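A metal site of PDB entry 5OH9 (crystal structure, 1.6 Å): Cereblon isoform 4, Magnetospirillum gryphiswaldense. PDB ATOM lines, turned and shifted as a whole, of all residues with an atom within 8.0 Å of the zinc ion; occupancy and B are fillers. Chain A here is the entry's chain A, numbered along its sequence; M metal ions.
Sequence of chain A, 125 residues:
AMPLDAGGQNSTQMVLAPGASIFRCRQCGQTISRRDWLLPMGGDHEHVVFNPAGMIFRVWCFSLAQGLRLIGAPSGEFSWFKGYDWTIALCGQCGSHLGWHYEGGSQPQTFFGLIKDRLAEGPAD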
ATOM      1  N   ARG A  24      -3.055 -24.865 -15.276  1.00  0.00           N
ATOM      2  CA  ARG A  24      -4.388 -24.376 -15.305  1.00  0.00           C
ATOM      3  C   ARG A  24      -4.427 -22.860 -15.132  1.00  0.00           C
ATOM      4  O   ARG A  24      -3.490 -22.286 -14.599  1.00  0.00           O
ATOM      5  CB  ARG A  24      -5.205 -25.035 -14.148  1.00  0.00           C
ATOM      6  CG  ARG A  24      -5.452 -26.498 -14.348  1.00  0.00           C
ATOM      7  CD  ARG A  24      -6.355 -27.109 -13.252  1.00  0.00           C
ATOM      8  NE  ARG A  24      -6.539 -28.509 -13.544  1.00  0.00           N
ATOM      9  CZ  ARG A  24      -7.368 -28.985 -14.444  1.00  0.00           C
ATOM     10  NH1 ARG A  24      -8.225 -28.191 -15.063  1.00  0.00           N
ATOM     11  NH2 ARG A  24      -7.413 -30.304 -14.679  1.00  0.00           N
ATOM     12  N   CYS A  25      -5.502 -22.218 -15.589  1.00  0.00           N
ATOM     13  CA  CYS A  25      -5.742 -20.808 -15.318  1.00  0.00           C
ATOM     14  C   CYS A  25      -5.779 -20.595 -13.795  1.00  0.00           C
ATOM     15  O   CYS A  25      -6.526 -21.234 -13.102  1.00  0.00           O
ATOM     16  CB  CYS A  25      -7.056 -20.350 -15.940  1.00  0.00           C
ATOM     17  SG  CYS A  25      -7.437 -18.603 -15.533  1.00  0.00           S
ATOM     18  N   ARG A  26      -4.964 -19.691 -13.281  1.00  0.00           N
ATOM     19  CA  ARG A  26      -4.911 -19.467 -11.849  1.00  0.00           C
ATOM     20  C   ARG A  26      -6.244 -18.901 -11.306  1.00  0.00           C
ATOM     21  O   ARG A  26      -6.598 -19.076 -10.117  1.00  0.00           O
ATOM     22  CB  ARG A  26      -3.726 -18.526 -11.548  1.00  0.00           C
ATOM     23  CG  ARG A  26      -3.634 -17.982 -10.184  1.00  0.00           C
ATOM     24  CD  ARG A  26      -2.440 -17.090 -10.052  1.00  0.00           C
ATOM     25  NE  ARG A  26      -2.424 -16.569  -8.729  1.00  0.00           N
ATOM     26  CZ  ARG A  26      -1.535 -15.730  -8.255  1.00  0.00           C
ATOM     27  NH1 ARG A  26      -0.515 -15.317  -9.030  1.00  0.00           N
ATOM     28  NH2 ARG A  26      -1.656 -15.334  -7.016  1.00  0.00           N
ATOM     29  N   GLN A  27      -6.948 -18.158 -12.167  1.00  0.00           N
ATOM     30  CA  GLN A  27      -8.168 -17.500 -11.744  1.00  0.00           C
ATOM     31  C   GLN A  27      -9.387 -18.389 -11.687  1.00  0.00           C
ATOM     32  O   GLN A  27     -10.305 -18.066 -10.910  1.00  0.00           O
ATOM     33  CB  GLN A  27      -8.443 -16.284 -12.608  1.00  0.00           C
ATOM     34  CG  GLN A  27      -7.365 -15.239 -12.448  1.00  0.00           C
ATOM     35  CD  GLN A  27      -7.128 -14.832 -10.992  1.00  0.00           C
ATOM     36  OE1 GLN A  27      -5.990 -14.894 -10.453  1.00  0.00           O
ATOM     37  NE2 GLN A  27      -8.193 -14.428 -10.318  1.00  0.00           N
ATOM     38  N   CYS A  28      -9.426 -19.478 -12.444  1.00  0.00           N
ATOM     39  CA  CYS A  28     -10.636 -20.288 -12.504  1.00  0.00           C
ATOM     40  C   CYS A  28     -10.434 -21.759 -12.606  1.00  0.00           C
ATOM     41  O   CYS A  28     -11.380 -22.512 -12.418  1.00  0.00           O
ATOM     42  CB  CYS A  28     -11.499 -19.803 -13.662  1.00  0.00           C
ATOM     43  SG  CYS A  28     -10.891 -20.286 -15.296  1.00  0.00           S
ATOM     44  N   GLY A  29      -9.227 -22.222 -12.976  1.00  0.00           N
ATOM     45  CA  GLY A  29      -9.000 -23.633 -13.127  1.00  0.00           C
ATOM     46  C   GLY A  29      -9.060 -24.266 -14.480  1.00  0.00           C
ATOM     47  O   GLY A  29      -8.752 -25.450 -14.635  1.00  0.00           O
ATOM     48  N   GLN A  30      -9.466 -23.491 -15.497  1.00  0.00           N
ATOM     49  CA  GLN A  30      -9.472 -23.957 -16.849  1.00  0.00           C
ATOM     50  C   GLN A  30      -8.144 -24.680 -17.219  1.00  0.00           C
ATOM     51  O   GLN A  30      -7.077 -24.156 -16.962  1.00  0.00           O
ATOM     52  CB  GLN A  30      -9.665 -22.736 -17.770  1.00  0.00           C
ATOM     53  CG  GLN A  30      -9.579 -23.010 -19.252  1.00  0.00           C
ATOM     54  CD  GLN A  30     -10.841 -23.619 -19.808  1.00  0.00           C
ATOM     55  OE1 GLN A  30     -11.500 -24.447 -19.181  1.00  0.00           O
ATOM     56  NE2 GLN A  30     -11.190 -23.197 -21.011  1.00  0.00           N
ATOM     57  N   THR A  31      -8.224 -25.846 -17.850  1.00  0.00           N
ATOM     58  CA  THR A  31      -7.007 -26.520 -18.316  1.00  0.00           C
ATOM     59  C   THR A  31      -6.390 -25.729 -19.488  1.00  0.00           C
ATOM     60  O   THR A  31      -7.096 -25.450 -20.434  1.00  0.00           O
ATOM     61  CB  THR A  31      -7.324 -27.942 -18.776  1.00  0.00           C
ATOM     62  OG1 THR A  31      -8.174 -28.592 -17.812  1.00  0.00           O
ATOM     63  CG2 THR A  31      -6.103 -28.717 -18.875  1.00  0.00           C
ATOM     64  N   ILE A  32      -5.090 -25.418 -19.421  1.00  0.00           N
ATOM     65  CA  ILE A  32      -4.428 -24.576 -20.437  1.00  0.00           C
ATOM     66  C   ILE A  32      -3.249 -25.247 -21.133  1.00  0.00           C
ATOM     67  O   ILE A  32      -3.193 -25.296 -22.359  1.00  0.00           O
ATOM     68  CB  ILE A  32      -3.948 -23.215 -19.893  1.00  0.00           C
ATOM     69  CG1 ILE A  32      -5.067 -22.450 -19.205  1.00  0.00           C
ATOM     70  CG2 ILE A  32      -3.295 -22.410 -20.987  1.00  0.00           C
ATOM     71  CD1 ILE A  32      -6.175 -22.020 -20.118  1.00  0.00           C
ATOM     72  N   GLY A  67      -7.886 -24.343 -24.276  1.00  0.00           N
ATOM     73  CA  GLY A  67      -8.774 -23.654 -23.332  1.00  0.00           C
ATOM     74  C   GLY A  67      -8.674 -22.150 -23.356  1.00  0.00           C
ATOM     75  O   GLY A  67      -9.152 -21.478 -22.429  1.00  0.00           O
ATOM     76  N   LEU A  68      -8.008 -21.629 -24.375  1.00  0.00           N
ATOM     77  CA  LEU A  68      -7.842 -20.201 -24.563  1.00  0.00           C
ATOM     78  C   LEU A  68      -8.870 -19.710 -25.551  1.00  0.00           C
ATOM     79  O   LEU A  68      -9.560 -20.494 -26.186  1.00  0.00           O
ATOM     80  CB  LEU A  68      -6.411 -19.872 -25.071  1.00  0.00           C
ATOM     81  CG  LEU A  68      -5.309 -20.294 -24.123  1.00  0.00           C
ATOM     82  CD1 LEU A  68      -4.006 -20.333 -24.923  1.00  0.00           C
ATOM     83  CD2 LEU A  68      -5.215 -19.384 -22.879  1.00  0.00           C
ATOM     84  N   LEU A  90      -6.806 -15.025 -24.195  1.00  0.00           N
ATOM     85  CA  LEU A  90      -7.553 -15.005 -22.945  1.00  0.00           C
ATOM     86  C   LEU A  90      -7.867 -16.446 -22.518  1.00  0.00           C
ATOM     87  O   LEU A  90      -8.017 -17.329 -23.349  1.00  0.00           O
ATOM     88  CB  LEU A  90      -8.858 -14.246 -23.105  1.00  0.00           C
ATOM     89  CG  LEU A  90      -8.795 -12.770 -23.596  1.00  0.00           C
ATOM     90  CD1 LEU A  90     -10.180 -12.175 -23.568  1.00  0.00           C
ATOM     91  CD2 LEU A  90      -7.753 -11.956 -22.810  1.00  0.00           C
ATOM     92  N   CYS A  91      -8.020 -16.642 -21.211  1.00  0.00           N
ATOM     93  CA  CYS A  91      -8.617 -17.848 -20.697  1.00  0.00           C
ATOM     94  C   CYS A  91      -9.998 -17.925 -21.360  1.00  0.00           C
ATOM     95  O   CYS A  91     -10.805 -16.982 -21.272  1.00  0.00           O
ATOM     96  CB  CYS A  91      -8.778 -17.787 -19.182  1.00  0.00           C
ATOM     97  SG  CYS A  91      -9.627 -19.250 -18.528  1.00  0.00           S
ATOM     98  N   GLY A  92     -10.311 -19.036 -22.030  1.00  0.00           N
ATOM     99  CA  GLY A  92     -11.594 -19.191 -22.657  1.00  0.00           C
ATOM    100  C   GLY A  92     -12.780 -19.285 -21.727  1.00  0.00           C
ATOM    101  O   GLY A  92     -13.935 -19.110 -22.125  1.00  0.00           O
ATOM    102  N   GLN A  93     -12.503 -19.607 -20.478  1.00  0.00           N
ATOM    103  CA  GLN A  93     -13.506 -19.771 -19.468  1.00  0.00           C
ATOM    104  C   GLN A  93     -13.793 -18.420 -18.763  1.00  0.00           C
ATOM    105  O   GLN A  93     -14.915 -17.938 -18.825  1.00  0.00           O
ATOM    106  CB  GLN A  93     -13.102 -20.845 -18.465  1.00  0.00           C
ATOM    107  CG  GLN A  93     -14.133 -21.183 -17.386  1.00  0.00           C
ATOM    108  CD  GLN A  93     -13.938 -22.556 -16.759  1.00  0.00           C
ATOM    109  OE1 GLN A  93     -14.546 -23.497 -17.198  1.00  0.00           O
ATOM    110  NE2 GLN A  93     -13.003 -22.664 -15.816  1.00  0.00           N
ATOM    111  N   CYS A  94     -12.784 -17.808 -18.161  1.00  0.00           N
ATOM    112  CA  CYS A  94     -13.009 -16.628 -17.321  1.00  0.00           C
ATOM    113  C   CYS A  94     -12.575 -15.290 -17.937  1.00  0.00           C
ATOM    114  O   CYS A  94     -12.938 -14.243 -17.397  1.00  0.00           O
ATOM    115  CB  CYS A  94     -12.320 -16.813 -15.974  1.00  0.00           C
ATOM    116  SG  CYS A  94     -10.521 -16.499 -15.951  1.00  0.00           S
ATOM    117  N   GLY A  95     -11.854 -15.302 -19.048  1.00  0.00           N
ATOM    118  CA  GLY A  95     -11.442 -14.077 -19.706  1.00  0.00           C
ATOM    119  C   GLY A  95     -10.152 -13.479 -19.194  1.00  0.00           C
ATOM    120  O   GLY A  95      -9.725 -12.443 -19.746  1.00  0.00           O
ATOM    121  N   SER A  96      -9.508 -14.100 -18.236  1.00  0.00           N
ATOM    122  CA  SER A  96      -8.184 -13.641 -17.747  1.00  0.00           C
ATOM    123  C   SER A  96      -7.158 -13.567 -18.863  1.00  0.00           C
ATOM    124  O   SER A  96      -7.073 -14.472 -19.708  1.00  0.00           O
ATOM    125  CB  SER A  96      -7.656 -14.604 -16.705  1.00  0.00           C
ATOM    126  OG  SER A  96      -6.388 -14.175 -16.203  1.00  0.00           O
ATOM    127  N   HIS A  97      -6.392 -12.466 -18.915  1.00  0.00           N
ATOM    128  CA  HIS A  97      -5.346 -12.412 -19.933  1.00  0.00           C
ATOM    129  C   HIS A  97      -4.200 -13.320 -19.593  1.00  0.00           C
ATOM    130  O   HIS A  97      -3.443 -13.044 -18.675  1.00  0.00           O
ATOM    131  CB  HIS A  97      -4.877 -10.975 -20.101  1.00  0.00           C
ATOM    132  CG  HIS A  97      -3.807 -10.838 -21.105  1.00  0.00           C
ATOM    133  ND1 HIS A  97      -2.873  -9.826 -21.056  1.00  0.00           N
ATOM    134  CD2 HIS A  97      -3.507 -11.579 -22.199  1.00  0.00           C
ATOM    135  CE1 HIS A  97      -2.028  -9.960 -22.066  1.00  0.00           C
ATOM    136  NE2 HIS A  97      -2.374 -11.026 -22.759  1.00  0.00           N
ATOM    137  N   LEU A  98      -4.047 -14.439 -20.299  1.00  0.00           N
ATOM    138  CA  LEU A  98      -3.060 -15.413 -20.006  1.00  0.00           C
ATOM    139  C   LEU A  98      -1.781 -15.331 -20.839  1.00  0.00           C
ATOM    140  O   LEU A  98      -0.792 -15.898 -20.488  1.00  0.00           O
ATOM    141  CB  LEU A  98      -3.636 -16.821 -20.119  1.00  0.00           C
ATOM    142  CG  LEU A  98      -4.744 -17.191 -19.132  1.00  0.00           C
ATOM    143  CD1 LEU A  98      -5.120 -18.638 -19.241  1.00  0.00           C
ATOM    144  CD2 LEU A  98      -4.378 -16.874 -17.698  1.00  0.00           C
ATOM    145  N   ARG A 118       0.237 -16.283 -14.104  1.00  0.00           N
ATOM    146  CA  ARG A 118      -1.208 -16.335 -14.262  1.00  0.00           C
ATOM    147  C   ARG A 118      -1.702 -17.782 -14.444  1.00  0.00           C
ATOM    148  O   ARG A 118      -2.896 -18.018 -14.719  1.00  0.00           O
ATOM    149  CB  ARG A 118      -1.657 -15.381 -15.347  1.00  0.00           C
ATOM    150  CG  ARG A 118      -1.118 -13.972 -15.090  1.00  0.00           C
ATOM    151  CD  ARG A 118      -1.732 -12.984 -16.048  1.00  0.00           C
ATOM    152  NE  ARG A 118      -1.096 -11.712 -15.823  1.00  0.00           N
ATOM    153  CZ  ARG A 118      -1.386 -10.623 -16.503  1.00  0.00           C
ATOM    154  NH1 ARG A 118      -2.324 -10.657 -17.439  1.00  0.00           N
ATOM    155  NH2 ARG A 118      -0.701  -9.518 -16.239  1.00  0.00           N
HETATM  156 ZN    ZN M   1      -9.603 -18.597 -16.275  1.00  0.00          ZN
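SG of Cys 25 binds the zinc ion. The zinc ion is bound by SG of Cys 94 (2.3 Å). SG of Cys 28 is bound to the zinc ion. The side-chain sulfur (SG) of Cys 91 binds the zinc ion (2.3 Å).
N of Cys 25 sits at hydrogen-bond distance from O of Gln 30. SG of Cys 25 lies close to N of Gln 27 (3.4 Å). SG of Cys 94 lies close to N of Ser 96 (3.5 Å). The backbone NH (N) of Gln 30 sits close to the side-chain sulfur (SG) of Cys 28 (3.5 Å). The side-chain sulfur (SG) of Cys 28 lies close to the side-chain amide nitrogen (NE2) of Gln 93, 3.2 Å away. The backbone NH (N) of Cys 91 is in hydrogen-bond range of the backbone carbonyl oxygen (O) of Ser 96 (2.8 Å). SG of Cys 91 sits close to N of Gln 93, at 3.5 Å.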
